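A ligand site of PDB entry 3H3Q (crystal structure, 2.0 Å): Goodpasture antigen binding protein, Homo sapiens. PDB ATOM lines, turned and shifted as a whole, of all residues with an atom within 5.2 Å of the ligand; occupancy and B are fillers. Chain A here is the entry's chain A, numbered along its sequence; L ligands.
The side-chain amide oxygen of Gln 124 is in hydrogen-bond range of the side-chain hydroxyl of Tyr 139 (2.7 Å). N of His 126 is in hydrogen-bond range of O of Arg 135. The side-chain carboxylate of Glu 103 is in hydrogen-bond range of the side-chain hydroxyl of Thr 105 (2.8 Å). The guanidinium group of Arg 99 is in hydrogen-bond range of the backbone carbonyl oxygen of Phe 93 (3.1 Å). The backbone NH (N) of Ala 178 sits at hydrogen-bond distance from the backbone carbonyl oxygen (O) of Asp 136 (2.8 Å). ND1 of His 126 lies within hydrogen-bond range of O of Thr 105. N of Gln 124 is in hydrogen-bond range of O of Val 137 (3.0 Å). The guanidinium group of Arg 99 is in hydrogen-bond range of the side-chain hydroxyl of Tyr 139 (3.1 Å).
The guanidinium group of Arg 99 sits close to an oxygen (O2) of the ligand (3.4 Å). OE1 of Glu 103 lies within hydrogen-bond range of O2 of the ligand (2.9 Å). OD1 of Asn 161 is in hydrogen-bond range of O3 of the ligand (2.8 Å). An oxygen (O1) of the ligand is in hydrogen-bond range of the side-chain hydroxyl (OH) of Tyr 210, at 2.7 Å. An oxygen (O2) of the ligand sits at hydrogen-bond distance from the side-chain amide nitrogen (NE2) of Gln 124 (3.4 Å).
Phe 93 touches the ligand (CZ to O1, 3.3 Å). Ile 106 touches the ligand. His 126 touches the ligand (NE2 to C8, 3.5 Å). Val 129 touches the ligand (CG2 to C20, 3.6 Å). Arg 135 touches the ligand. OH of Tyr 139 touches C4 of the ligand (3.6 Å). Ala 178 touches the ligand. Ile 180 touches the ligand (CD1 to C6, 3.96 Å). Val 182 touches the ligand (CG1 to O3, 3.5 Å). Val 214 touches the ligand (CG2 to C10, 3.8 Å). CE1 of Tyr 233 touches C15 of the ligand, at 3.7 Å. CG of Phe 236 touches C14 of the ligand, 3.7 Å away. Hydrophobic or aromatic side chains that line the ligand: Phe 93, Ile 106, His 126, Val 129, Tyr 139, Ala 178, Ile 180, Val 182, Tyr 210, Val 214, Tyr 233 and Phe 236.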
ATOM      1  N   PHE A  93       6.243  -9.478 -18.946  1.00  0.00           N
ATOM      2  CA  PHE A  93       5.142  -8.587 -19.306  1.00  0.00           C
ATOM      3  C   PHE A  93       3.996  -9.322 -19.985  1.00  0.00           C
ATOM      4  O   PHE A  93       2.834  -8.979 -19.751  1.00  0.00           O
ATOM      5  CB  PHE A  93       5.612  -7.444 -20.219  1.00  0.00           C
ATOM      6  CG  PHE A  93       4.550  -6.393 -20.479  1.00  0.00           C
ATOM      7  CD1 PHE A  93       3.993  -5.664 -19.420  1.00  0.00           C
ATOM      8  CD2 PHE A  93       4.128  -6.125 -21.760  1.00  0.00           C
ATOM      9  CE1 PHE A  93       3.014  -4.685 -19.625  1.00  0.00           C
ATOM     10  CE2 PHE A  93       3.137  -5.132 -21.986  1.00  0.00           C
ATOM     11  CZ  PHE A  93       2.599  -4.406 -20.912  1.00  0.00           C
ATOM     12  N   ARG A  99       0.611 -12.417 -14.249  1.00  0.00           N
ATOM     13  CA  ARG A  99      -0.021 -11.093 -14.314  1.00  0.00           C
ATOM     14  C   ARG A  99      -0.459 -10.530 -12.953  1.00  0.00           C
ATOM     15  O   ARG A  99      -0.272  -9.343 -12.639  1.00  0.00           O
ATOM     16  CB  ARG A  99      -1.208 -11.143 -15.279  1.00  0.00           C
ATOM     17  CG  ARG A  99      -2.120  -9.897 -15.271  1.00  0.00           C
ATOM     18  CD  ARG A  99      -1.660  -8.881 -16.309  1.00  0.00           C
ATOM     19  NE  ARG A  99      -0.744  -9.529 -17.236  1.00  0.00           N
ATOM     20  CZ  ARG A  99      -0.908  -9.616 -18.557  1.00  0.00           C
ATOM     21  NH1 ARG A  99       0.013 -10.205 -19.276  1.00  0.00           N
ATOM     22  NH2 ARG A  99      -1.957  -9.078 -19.142  1.00  0.00           N
ATOM     23  N   TRP A 102       1.897  -8.584 -10.453  1.00  0.00           N
ATOM     24  CA  TRP A 102       2.344  -7.201 -10.554  1.00  0.00           C
ATOM     25  C   TRP A 102       1.251  -6.217 -10.938  1.00  0.00           C
ATOM     26  O   TRP A 102       1.265  -5.087 -10.492  1.00  0.00           O
ATOM     27  CB  TRP A 102       3.554  -7.074 -11.523  1.00  0.00           C
ATOM     28  CG  TRP A 102       3.271  -7.616 -12.899  1.00  0.00           C
ATOM     29  CD1 TRP A 102       3.500  -8.897 -13.356  1.00  0.00           C
ATOM     30  CD2 TRP A 102       2.688  -6.892 -13.987  1.00  0.00           C
ATOM     31  NE1 TRP A 102       3.080  -8.996 -14.673  1.00  0.00           N
ATOM     32  CE2 TRP A 102       2.592  -7.778 -15.088  1.00  0.00           C
ATOM     33  CE3 TRP A 102       2.244  -5.585 -14.153  1.00  0.00           C
ATOM     34  CZ2 TRP A 102       2.048  -7.391 -16.308  1.00  0.00           C
ATOM     35  CZ3 TRP A 102       1.687  -5.219 -15.361  1.00  0.00           C
ATOM     36  CH2 TRP A 102       1.594  -6.115 -16.414  1.00  0.00           C
ATOM     37  N   GLU A 103       0.312  -6.648 -11.769  1.00  0.00           N
ATOM     38  CA  GLU A 103      -0.752  -5.760 -12.236  1.00  0.00           C
ATOM     39  C   GLU A 103      -1.769  -5.414 -11.126  1.00  0.00           C
ATOM     40  O   GLU A 103      -2.236  -6.285 -10.422  1.00  0.00           O
ATOM     41  CB  GLU A 103      -1.416  -6.363 -13.489  1.00  0.00           C
ATOM     42  CG  GLU A 103      -2.642  -5.670 -13.978  1.00  0.00           C
ATOM     43  CD  GLU A 103      -2.383  -4.326 -14.600  1.00  0.00           C
ATOM     44  OE1 GLU A 103      -2.175  -4.277 -15.837  1.00  0.00           O
ATOM     45  OE2 GLU A 103      -2.461  -3.316 -13.877  1.00  0.00           O
ATOM     46  N   THR A 105      -4.447  -2.774 -11.626  1.00  0.00           N
ATOM     47  CA  THR A 105      -5.529  -1.940 -12.079  1.00  0.00           C
ATOM     48  C   THR A 105      -6.678  -2.753 -12.627  1.00  0.00           C
ATOM     49  O   THR A 105      -7.643  -2.179 -13.147  1.00  0.00           O
ATOM     50  CB  THR A 105      -5.131  -0.959 -13.204  1.00  0.00           C
ATOM     51  OG1 THR A 105      -4.741  -1.704 -14.377  1.00  0.00           O
ATOM     52  CG2 THR A 105      -4.041   0.024 -12.768  1.00  0.00           C
ATOM     53  N   ILE A 106      -6.542  -4.066 -12.560  1.00  0.00           N
ATOM     54  CA  ILE A 106      -7.463  -4.995 -13.183  1.00  0.00           C
ATOM     55  C   ILE A 106      -8.424  -5.552 -12.110  1.00  0.00           C
ATOM     56  O   ILE A 106      -8.005  -5.832 -10.974  1.00  0.00           O
ATOM     57  CB  ILE A 106      -6.698  -6.162 -13.795  1.00  0.00           C
ATOM     58  CG1 ILE A 106      -6.227  -5.831 -15.213  1.00  0.00           C
ATOM     59  CG2 ILE A 106      -7.548  -7.399 -13.896  1.00  0.00           C
ATOM     60  CD1 ILE A 106      -5.340  -6.943 -15.772  1.00  0.00           C
ATOM     61  N   GLN A 124     -10.506  -8.158 -20.289  1.00  0.00           N
ATOM     62  CA  GLN A 124     -10.297  -7.811 -18.893  1.00  0.00           C
ATOM     63  C   GLN A 124     -11.063  -6.580 -18.509  1.00  0.00           C
ATOM     64  O   GLN A 124     -11.412  -5.810 -19.386  1.00  0.00           O
ATOM     65  CB  GLN A 124      -8.804  -7.646 -18.566  1.00  0.00           C
ATOM     66  CG  GLN A 124      -8.130  -6.426 -19.230  1.00  0.00           C
ATOM     67  CD  GLN A 124      -6.635  -6.474 -19.095  1.00  0.00           C
ATOM     68  OE1 GLN A 124      -6.037  -7.509 -19.263  1.00  0.00           O
ATOM     69  NE2 GLN A 124      -6.037  -5.357 -18.770  1.00  0.00           N
ATOM     70  N   HIS A 126     -11.275  -3.139 -15.857  1.00  0.00           N
ATOM     71  CA  HIS A 126     -10.389  -2.405 -14.979  1.00  0.00           C
ATOM     72  C   HIS A 126     -11.123  -1.810 -13.749  1.00  0.00           C
ATOM     73  O   HIS A 126     -12.311  -1.466 -13.813  1.00  0.00           O
ATOM     74  CB  HIS A 126      -9.563  -1.354 -15.770  1.00  0.00           C
ATOM     75  CG  HIS A 126      -8.520  -1.972 -16.660  1.00  0.00           C
ATOM     76  ND1 HIS A 126      -7.241  -2.243 -16.237  1.00  0.00           N
ATOM     77  CD2 HIS A 126      -8.603  -2.427 -17.927  1.00  0.00           C
ATOM     78  CE1 HIS A 126      -6.570  -2.838 -17.209  1.00  0.00           C
ATOM     79  NE2 HIS A 126      -7.380  -2.955 -18.251  1.00  0.00           N
ATOM     80  N   VAL A 129     -10.495   3.410 -11.763  1.00  0.00           N
ATOM     81  CA  VAL A 129      -9.482   4.415 -11.472  1.00  0.00           C
ATOM     82  C   VAL A 129      -9.926   5.804 -11.977  1.00  0.00           C
ATOM     83  O   VAL A 129      -9.337   6.828 -11.628  1.00  0.00           O
ATOM     84  CB  VAL A 129      -8.087   3.984 -12.034  1.00  0.00           C
ATOM     85  CG1 VAL A 129      -7.703   2.581 -11.520  1.00  0.00           C
ATOM     86  CG2 VAL A 129      -8.087   3.988 -13.564  1.00  0.00           C
ATOM     87  N   TRP A 130     -10.966   5.834 -12.805  1.00  0.00           N
ATOM     88  CA  TRP A 130     -11.487   7.107 -13.316  1.00  0.00           C
ATOM     89  C   TRP A 130     -12.816   7.537 -12.646  1.00  0.00           C
ATOM     90  O   TRP A 130     -13.555   6.676 -12.144  1.00  0.00           O
ATOM     91  CB  TRP A 130     -11.676   7.019 -14.845  1.00  0.00           C
ATOM     92  CG  TRP A 130     -10.370   6.890 -15.608  1.00  0.00           C
ATOM     93  CD1 TRP A 130      -9.122   7.345 -15.212  1.00  0.00           C
ATOM     94  CD2 TRP A 130     -10.182   6.278 -16.897  1.00  0.00           C
ATOM     95  NE1 TRP A 130      -8.185   7.030 -16.182  1.00  0.00           N
ATOM     96  CE2 TRP A 130      -8.803   6.382 -17.221  1.00  0.00           C
ATOM     97  CE3 TRP A 130     -11.046   5.657 -17.811  1.00  0.00           C
ATOM     98  CZ2 TRP A 130      -8.275   5.887 -18.428  1.00  0.00           C
ATOM     99  CZ3 TRP A 130     -10.523   5.164 -19.005  1.00  0.00           C
ATOM    100  CH2 TRP A 130      -9.144   5.286 -19.301  1.00  0.00           C
ATOM    101  N   ARG A 135     -14.463   0.541 -17.207  1.00  0.00           N
ATOM    102  CA  ARG A 135     -13.984   0.140 -18.551  1.00  0.00           C
ATOM    103  C   ARG A 135     -13.601  -1.314 -18.639  1.00  0.00           C
ATOM    104  O   ARG A 135     -13.129  -1.914 -17.670  1.00  0.00           O
ATOM    105  CB  ARG A 135     -12.762   0.962 -18.935  1.00  0.00           C
ATOM    106  CG  ARG A 135     -13.078   2.148 -19.738  1.00  0.00           C
ATOM    107  CD  ARG A 135     -13.997   3.034 -18.972  1.00  0.00           C
ATOM    108  NE  ARG A 135     -14.232   4.265 -19.713  1.00  0.00           N
ATOM    109  CZ  ARG A 135     -15.224   5.111 -19.463  1.00  0.00           C
ATOM    110  NH1 ARG A 135     -16.069   4.839 -18.483  1.00  0.00           N
ATOM    111  NH2 ARG A 135     -15.360   6.210 -20.203  1.00  0.00           N
ATOM    112  N   ASP A 136     -13.814  -1.888 -19.817  1.00  0.00           N
ATOM    113  CA  ASP A 136     -13.154  -3.139 -20.169  1.00  0.00           C
ATOM    114  C   ASP A 136     -12.414  -2.951 -21.498  1.00  0.00           C
ATOM    115  O   ASP A 136     -12.562  -1.931 -22.149  1.00  0.00           O
ATOM    116  CB  ASP A 136     -14.105  -4.342 -20.236  1.00  0.00           C
ATOM    117  CG  ASP A 136     -15.226  -4.147 -21.222  1.00  0.00           C
ATOM    118  OD1 ASP A 136     -15.314  -3.091 -21.878  1.00  0.00           O
ATOM    119  OD2 ASP A 136     -16.048  -5.066 -21.307  1.00  0.00           O
ATOM    120  N   VAL A 137     -11.627  -3.961 -21.864  1.00  0.00           N
ATOM    121  CA  VAL A 137     -10.731  -3.891 -23.005  1.00  0.00           C
ATOM    122  C   VAL A 137     -10.593  -5.322 -23.462  1.00  0.00           C
ATOM    123  O   VAL A 137     -10.606  -6.232 -22.650  1.00  0.00           O
ATOM    124  CB  VAL A 137      -9.351  -3.282 -22.594  1.00  0.00           C
ATOM    125  CG1 VAL A 137      -8.610  -4.228 -21.685  1.00  0.00           C
ATOM    126  CG2 VAL A 137      -8.499  -2.917 -23.828  1.00  0.00           C
ATOM    127  N   TYR A 139      -8.070  -7.376 -26.230  1.00  0.00           N
ATOM    128  CA  TYR A 139      -6.829  -7.091 -27.002  1.00  0.00           C
ATOM    129  C   TYR A 139      -6.037  -8.314 -27.331  1.00  0.00           C
ATOM    130  O   TYR A 139      -6.020  -9.289 -26.568  1.00  0.00           O
ATOM    131  CB  TYR A 139      -5.918  -6.103 -26.246  1.00  0.00           C
ATOM    132  CG  TYR A 139      -5.410  -6.560 -24.870  1.00  0.00           C
ATOM    133  CD1 TYR A 139      -4.150  -7.109 -24.722  1.00  0.00           C
ATOM    134  CD2 TYR A 139      -6.204  -6.432 -23.717  1.00  0.00           C
ATOM    135  CE1 TYR A 139      -3.679  -7.515 -23.451  1.00  0.00           C
ATOM    136  CE2 TYR A 139      -5.743  -6.838 -22.441  1.00  0.00           C
ATOM    137  CZ  TYR A 139      -4.484  -7.366 -22.334  1.00  0.00           C
ATOM    138  OH  TYR A 139      -4.037  -7.806 -21.098  1.00  0.00           O
ATOM    139  N   ASN A 161       0.222  -4.854 -27.202  1.00  0.00           N
ATOM    140  CA  ASN A 161      -1.163  -5.107 -26.732  1.00  0.00           C
ATOM    141  C   ASN A 161      -2.037  -4.142 -27.496  1.00  0.00           C
ATOM    142  O   ASN A 161      -1.925  -2.938 -27.304  1.00  0.00           O
ATOM    143  CB  ASN A 161      -1.332  -4.834 -25.233  1.00  0.00           C
ATOM    144  CG  ASN A 161      -0.597  -5.812 -24.367  1.00  0.00           C
ATOM    145  OD1 ASN A 161      -0.277  -5.511 -23.213  1.00  0.00           O
ATOM    146  ND2 ASN A 161      -0.302  -6.978 -24.906  1.00  0.00           N
ATOM    147  N   ALA A 178     -12.988   0.357 -23.659  1.00  0.00           N
ATOM    148  CA  ALA A 178     -11.766   1.105 -23.996  1.00  0.00           C
ATOM    149  C   ALA A 178     -11.043   0.462 -25.193  1.00  0.00           C
ATOM    150  O   ALA A 178     -11.179  -0.721 -25.451  1.00  0.00           O
ATOM    151  CB  ALA A 178     -10.833   1.163 -22.747  1.00  0.00           C
ATOM    152  N   ILE A 180      -7.053   0.139 -26.894  1.00  0.00           N
ATOM    153  CA  ILE A 180      -5.654   0.418 -26.609  1.00  0.00           C
ATOM    154  C   ILE A 180      -4.703   0.111 -27.750  1.00  0.00           C
ATOM    155  O   ILE A 180      -4.908  -0.790 -28.555  1.00  0.00           O
ATOM    156  CB  ILE A 180      -5.161  -0.327 -25.324  1.00  0.00           C
ATOM    157  CG1 ILE A 180      -5.275  -1.845 -25.500  1.00  0.00           C
ATOM    158  CG2 ILE A 180      -6.004   0.120 -24.108  1.00  0.00           C
ATOM    159  CD1 ILE A 180      -4.553  -2.638 -24.359  1.00  0.00           C
ATOM    160  N   VAL A 182      -0.626  -0.477 -27.215  1.00  0.00           N
ATOM    161  CA  VAL A 182       0.406  -0.402 -26.190  1.00  0.00           C
ATOM    162  C   VAL A 182       1.567  -1.249 -26.641  1.00  0.00           C
ATOM    163  O   VAL A 182       1.393  -2.281 -27.313  1.00  0.00           O
ATOM    164  CB  VAL A 182      -0.134  -0.929 -24.766  1.00  0.00           C
ATOM    165  CG1 VAL A 182       1.004  -1.134 -23.749  1.00  0.00           C
ATOM    166  CG2 VAL A 182      -1.136   0.042 -24.186  1.00  0.00           C
ATOM    167  N   TYR A 210       8.233   2.125 -23.184  1.00  0.00           N
ATOM    168  CA  TYR A 210       6.869   1.670 -23.022  1.00  0.00           C
ATOM    169  C   TYR A 210       5.959   2.764 -23.550  1.00  0.00           C
ATOM    170  O   TYR A 210       6.016   3.888 -23.087  1.00  0.00           O
ATOM    171  CB  TYR A 210       6.595   1.436 -21.543  1.00  0.00           C
ATOM    172  CG  TYR A 210       5.169   1.175 -21.247  1.00  0.00           C
ATOM    173  CD1 TYR A 210       4.295   2.180 -20.852  1.00  0.00           C
ATOM    174  CD2 TYR A 210       4.677  -0.111 -21.320  1.00  0.00           C
ATOM    175  CE1 TYR A 210       2.931   1.872 -20.557  1.00  0.00           C
ATOM    176  CE2 TYR A 210       3.360  -0.404 -21.017  1.00  0.00           C
ATOM    177  CZ  TYR A 210       2.507   0.554 -20.661  1.00  0.00           C
ATOM    178  OH  TYR A 210       1.219   0.113 -20.389  1.00  0.00           O
ATOM    179  N   ALA A 212       1.851   3.894 -24.463  1.00  0.00           N
ATOM    180  CA  ALA A 212       0.447   3.488 -24.276  1.00  0.00           C
ATOM    181  C   ALA A 212      -0.446   4.516 -24.926  1.00  0.00           C
ATOM    182  O   ALA A 212      -0.360   5.681 -24.594  1.00  0.00           O
ATOM    183  CB  ALA A 212       0.114   3.360 -22.818  1.00  0.00           C
ATOM    184  N   VAL A 214      -4.365   4.935 -25.129  1.00  0.00           N
ATOM    185  CA  VAL A 214      -5.629   4.407 -24.608  1.00  0.00           C
ATOM    186  C   VAL A 214      -6.758   5.373 -24.935  1.00  0.00           C
ATOM    187  O   VAL A 214      -6.659   6.578 -24.680  1.00  0.00           O
ATOM    188  CB  VAL A 214      -5.534   4.216 -23.080  1.00  0.00           C
ATOM    189  CG1 VAL A 214      -6.860   3.680 -22.482  1.00  0.00           C
ATOM    190  CG2 VAL A 214      -4.330   3.298 -22.722  1.00  0.00           C
ATOM    191  N   GLU A 232      -0.591   6.402 -12.083  1.00  0.00           N
ATOM    192  CA  GLU A 232      -0.686   4.968 -12.331  1.00  0.00           C
ATOM    193  C   GLU A 232       0.373   4.340 -13.237  1.00  0.00           C
ATOM    194  O   GLU A 232       0.844   3.253 -12.974  1.00  0.00           O
ATOM    195  CB  GLU A 232      -2.082   4.597 -12.839  1.00  0.00           C
ATOM    196  CG  GLU A 232      -3.187   4.779 -11.839  1.00  0.00           C
ATOM    197  CD  GLU A 232      -2.990   3.945 -10.608  1.00  0.00           C
ATOM    198  OE1 GLU A 232      -2.675   2.751 -10.732  1.00  0.00           O
ATOM    199  OE2 GLU A 232      -3.113   4.513  -9.495  1.00  0.00           O
ATOM    200  N   TYR A 233       0.754   4.995 -14.334  1.00  0.00           N
ATOM    201  CA  TYR A 233       1.860   4.472 -15.160  1.00  0.00           C
ATOM    202  C   TYR A 233       3.221   4.358 -14.459  1.00  0.00           C
ATOM    203  O   TYR A 233       3.856   3.306 -14.512  1.00  0.00           O
ATOM    204  CB  TYR A 233       1.985   5.291 -16.451  1.00  0.00           C
ATOM    205  CG  TYR A 233       0.851   4.982 -17.408  1.00  0.00           C
ATOM    206  CD1 TYR A 233       0.814   3.792 -18.098  1.00  0.00           C
ATOM    207  CD2 TYR A 233      -0.181   5.898 -17.601  1.00  0.00           C
ATOM    208  CE1 TYR A 233      -0.197   3.493 -18.965  1.00  0.00           C
ATOM    209  CE2 TYR A 233      -1.207   5.622 -18.491  1.00  0.00           C
ATOM    210  CZ  TYR A 233      -1.204   4.405 -19.156  1.00  0.00           C
ATOM    211  OH  TYR A 233      -2.199   4.113 -20.010  1.00  0.00           O
ATOM    212  N   PHE A 236       3.041   1.475 -11.989  1.00  0.00           N
ATOM    213  CA  PHE A 236       3.144   0.206 -12.716  1.00  0.00           C
ATOM    214  C   PHE A 236       4.588  -0.104 -13.123  1.00  0.00           C
ATOM    215  O   PHE A 236       5.106  -1.194 -12.834  1.00  0.00           O
ATOM    216  CB  PHE A 236       2.204   0.233 -13.955  1.00  0.00           C
ATOM    217  CG  PHE A 236       2.772  -0.457 -15.182  1.00  0.00           C
ATOM    218  CD1 PHE A 236       3.077  -1.803 -15.169  1.00  0.00           C
ATOM    219  CD2 PHE A 236       2.975   0.258 -16.369  1.00  0.00           C
ATOM    220  CE1 PHE A 236       3.589  -2.430 -16.289  1.00  0.00           C
ATOM    221  CE2 PHE A 236       3.472  -0.364 -17.495  1.00  0.00           C
ATOM    222  CZ  PHE A 236       3.785  -1.703 -17.465  1.00  0.00           C
HETATM  223  O1  LIG L   1       0.240  -2.344 -19.795  1.00  0.00           O
HETATM  224  C1  LIG L   1      -0.366  -2.703 -18.767  1.00  0.00           C
HETATM  225  N1  LIG L   1      -1.199  -3.769 -18.647  1.00  0.00           N
HETATM  226  C2  LIG L   1      -1.315  -4.838 -19.642  1.00  0.00           C
HETATM  227  C3  LIG L   1      -1.575  -6.138 -18.919  1.00  0.00           C
HETATM  228  O2  LIG L   1      -2.784  -5.937 -18.189  1.00  0.00           O
HETATM  229  C4  LIG L   1      -2.527  -4.538 -20.531  1.00  0.00           C
HETATM  230  C5  LIG L   1      -2.197  -3.141 -20.997  1.00  0.00           C
HETATM  231  C6  LIG L   1      -3.107  -1.964 -20.737  1.00  0.00           C
HETATM  232  C7  LIG L   1      -4.398  -2.064 -20.258  1.00  0.00           C
HETATM  233  C8  LIG L   1      -5.109  -0.908 -19.943  1.00  0.00           C
HETATM  234  C9  LIG L   1      -4.520   0.336 -20.071  1.00  0.00           C
HETATM  235  C10 LIG L   1      -3.197   0.438 -20.530  1.00  0.00           C
HETATM  236  C11 LIG L   1      -2.512  -0.710 -20.826  1.00  0.00           C
HETATM  237  O3  LIG L   1      -1.268  -3.147 -22.092  1.00  0.00           O
HETATM  238  C12 LIG L   1      -0.157  -1.911 -17.512  1.00  0.00           C
HETATM  239  C13 LIG L   1      -0.836  -0.567 -17.620  1.00  0.00           C
HETATM  240  C14 LIG L   1      -0.760   0.080 -16.244  1.00  0.00           C
HETATM  241  C15 LIG L   1      -1.392   1.464 -16.134  1.00  0.00           C
HETATM  242  C16 LIG L   1      -2.829   1.452 -16.596  1.00  0.00           C
HETATM  243  C17 LIG L   1      -3.525   2.720 -16.176  1.00  0.00           C
HETATM  244  C18 LIG L   1      -4.978   2.343 -15.897  1.00  0.00           C
HETATM  245  C19 LIG L   1      -5.985   3.013 -16.833  1.00  0.00           C
HETATM  246  C20 LIG L   1      -7.367   2.340 -16.726  1.00  0.00           C
HETATM  247  C21 LIG L   1      -7.571   1.301 -17.819  1.00  0.00           C
HETATM  248  C22 LIG L   1      -9.019   1.259 -18.312  1.00  0.00           C
HETATM  249  C23 LIG L   1      -9.071   0.892 -19.783  1.00  0.00           C
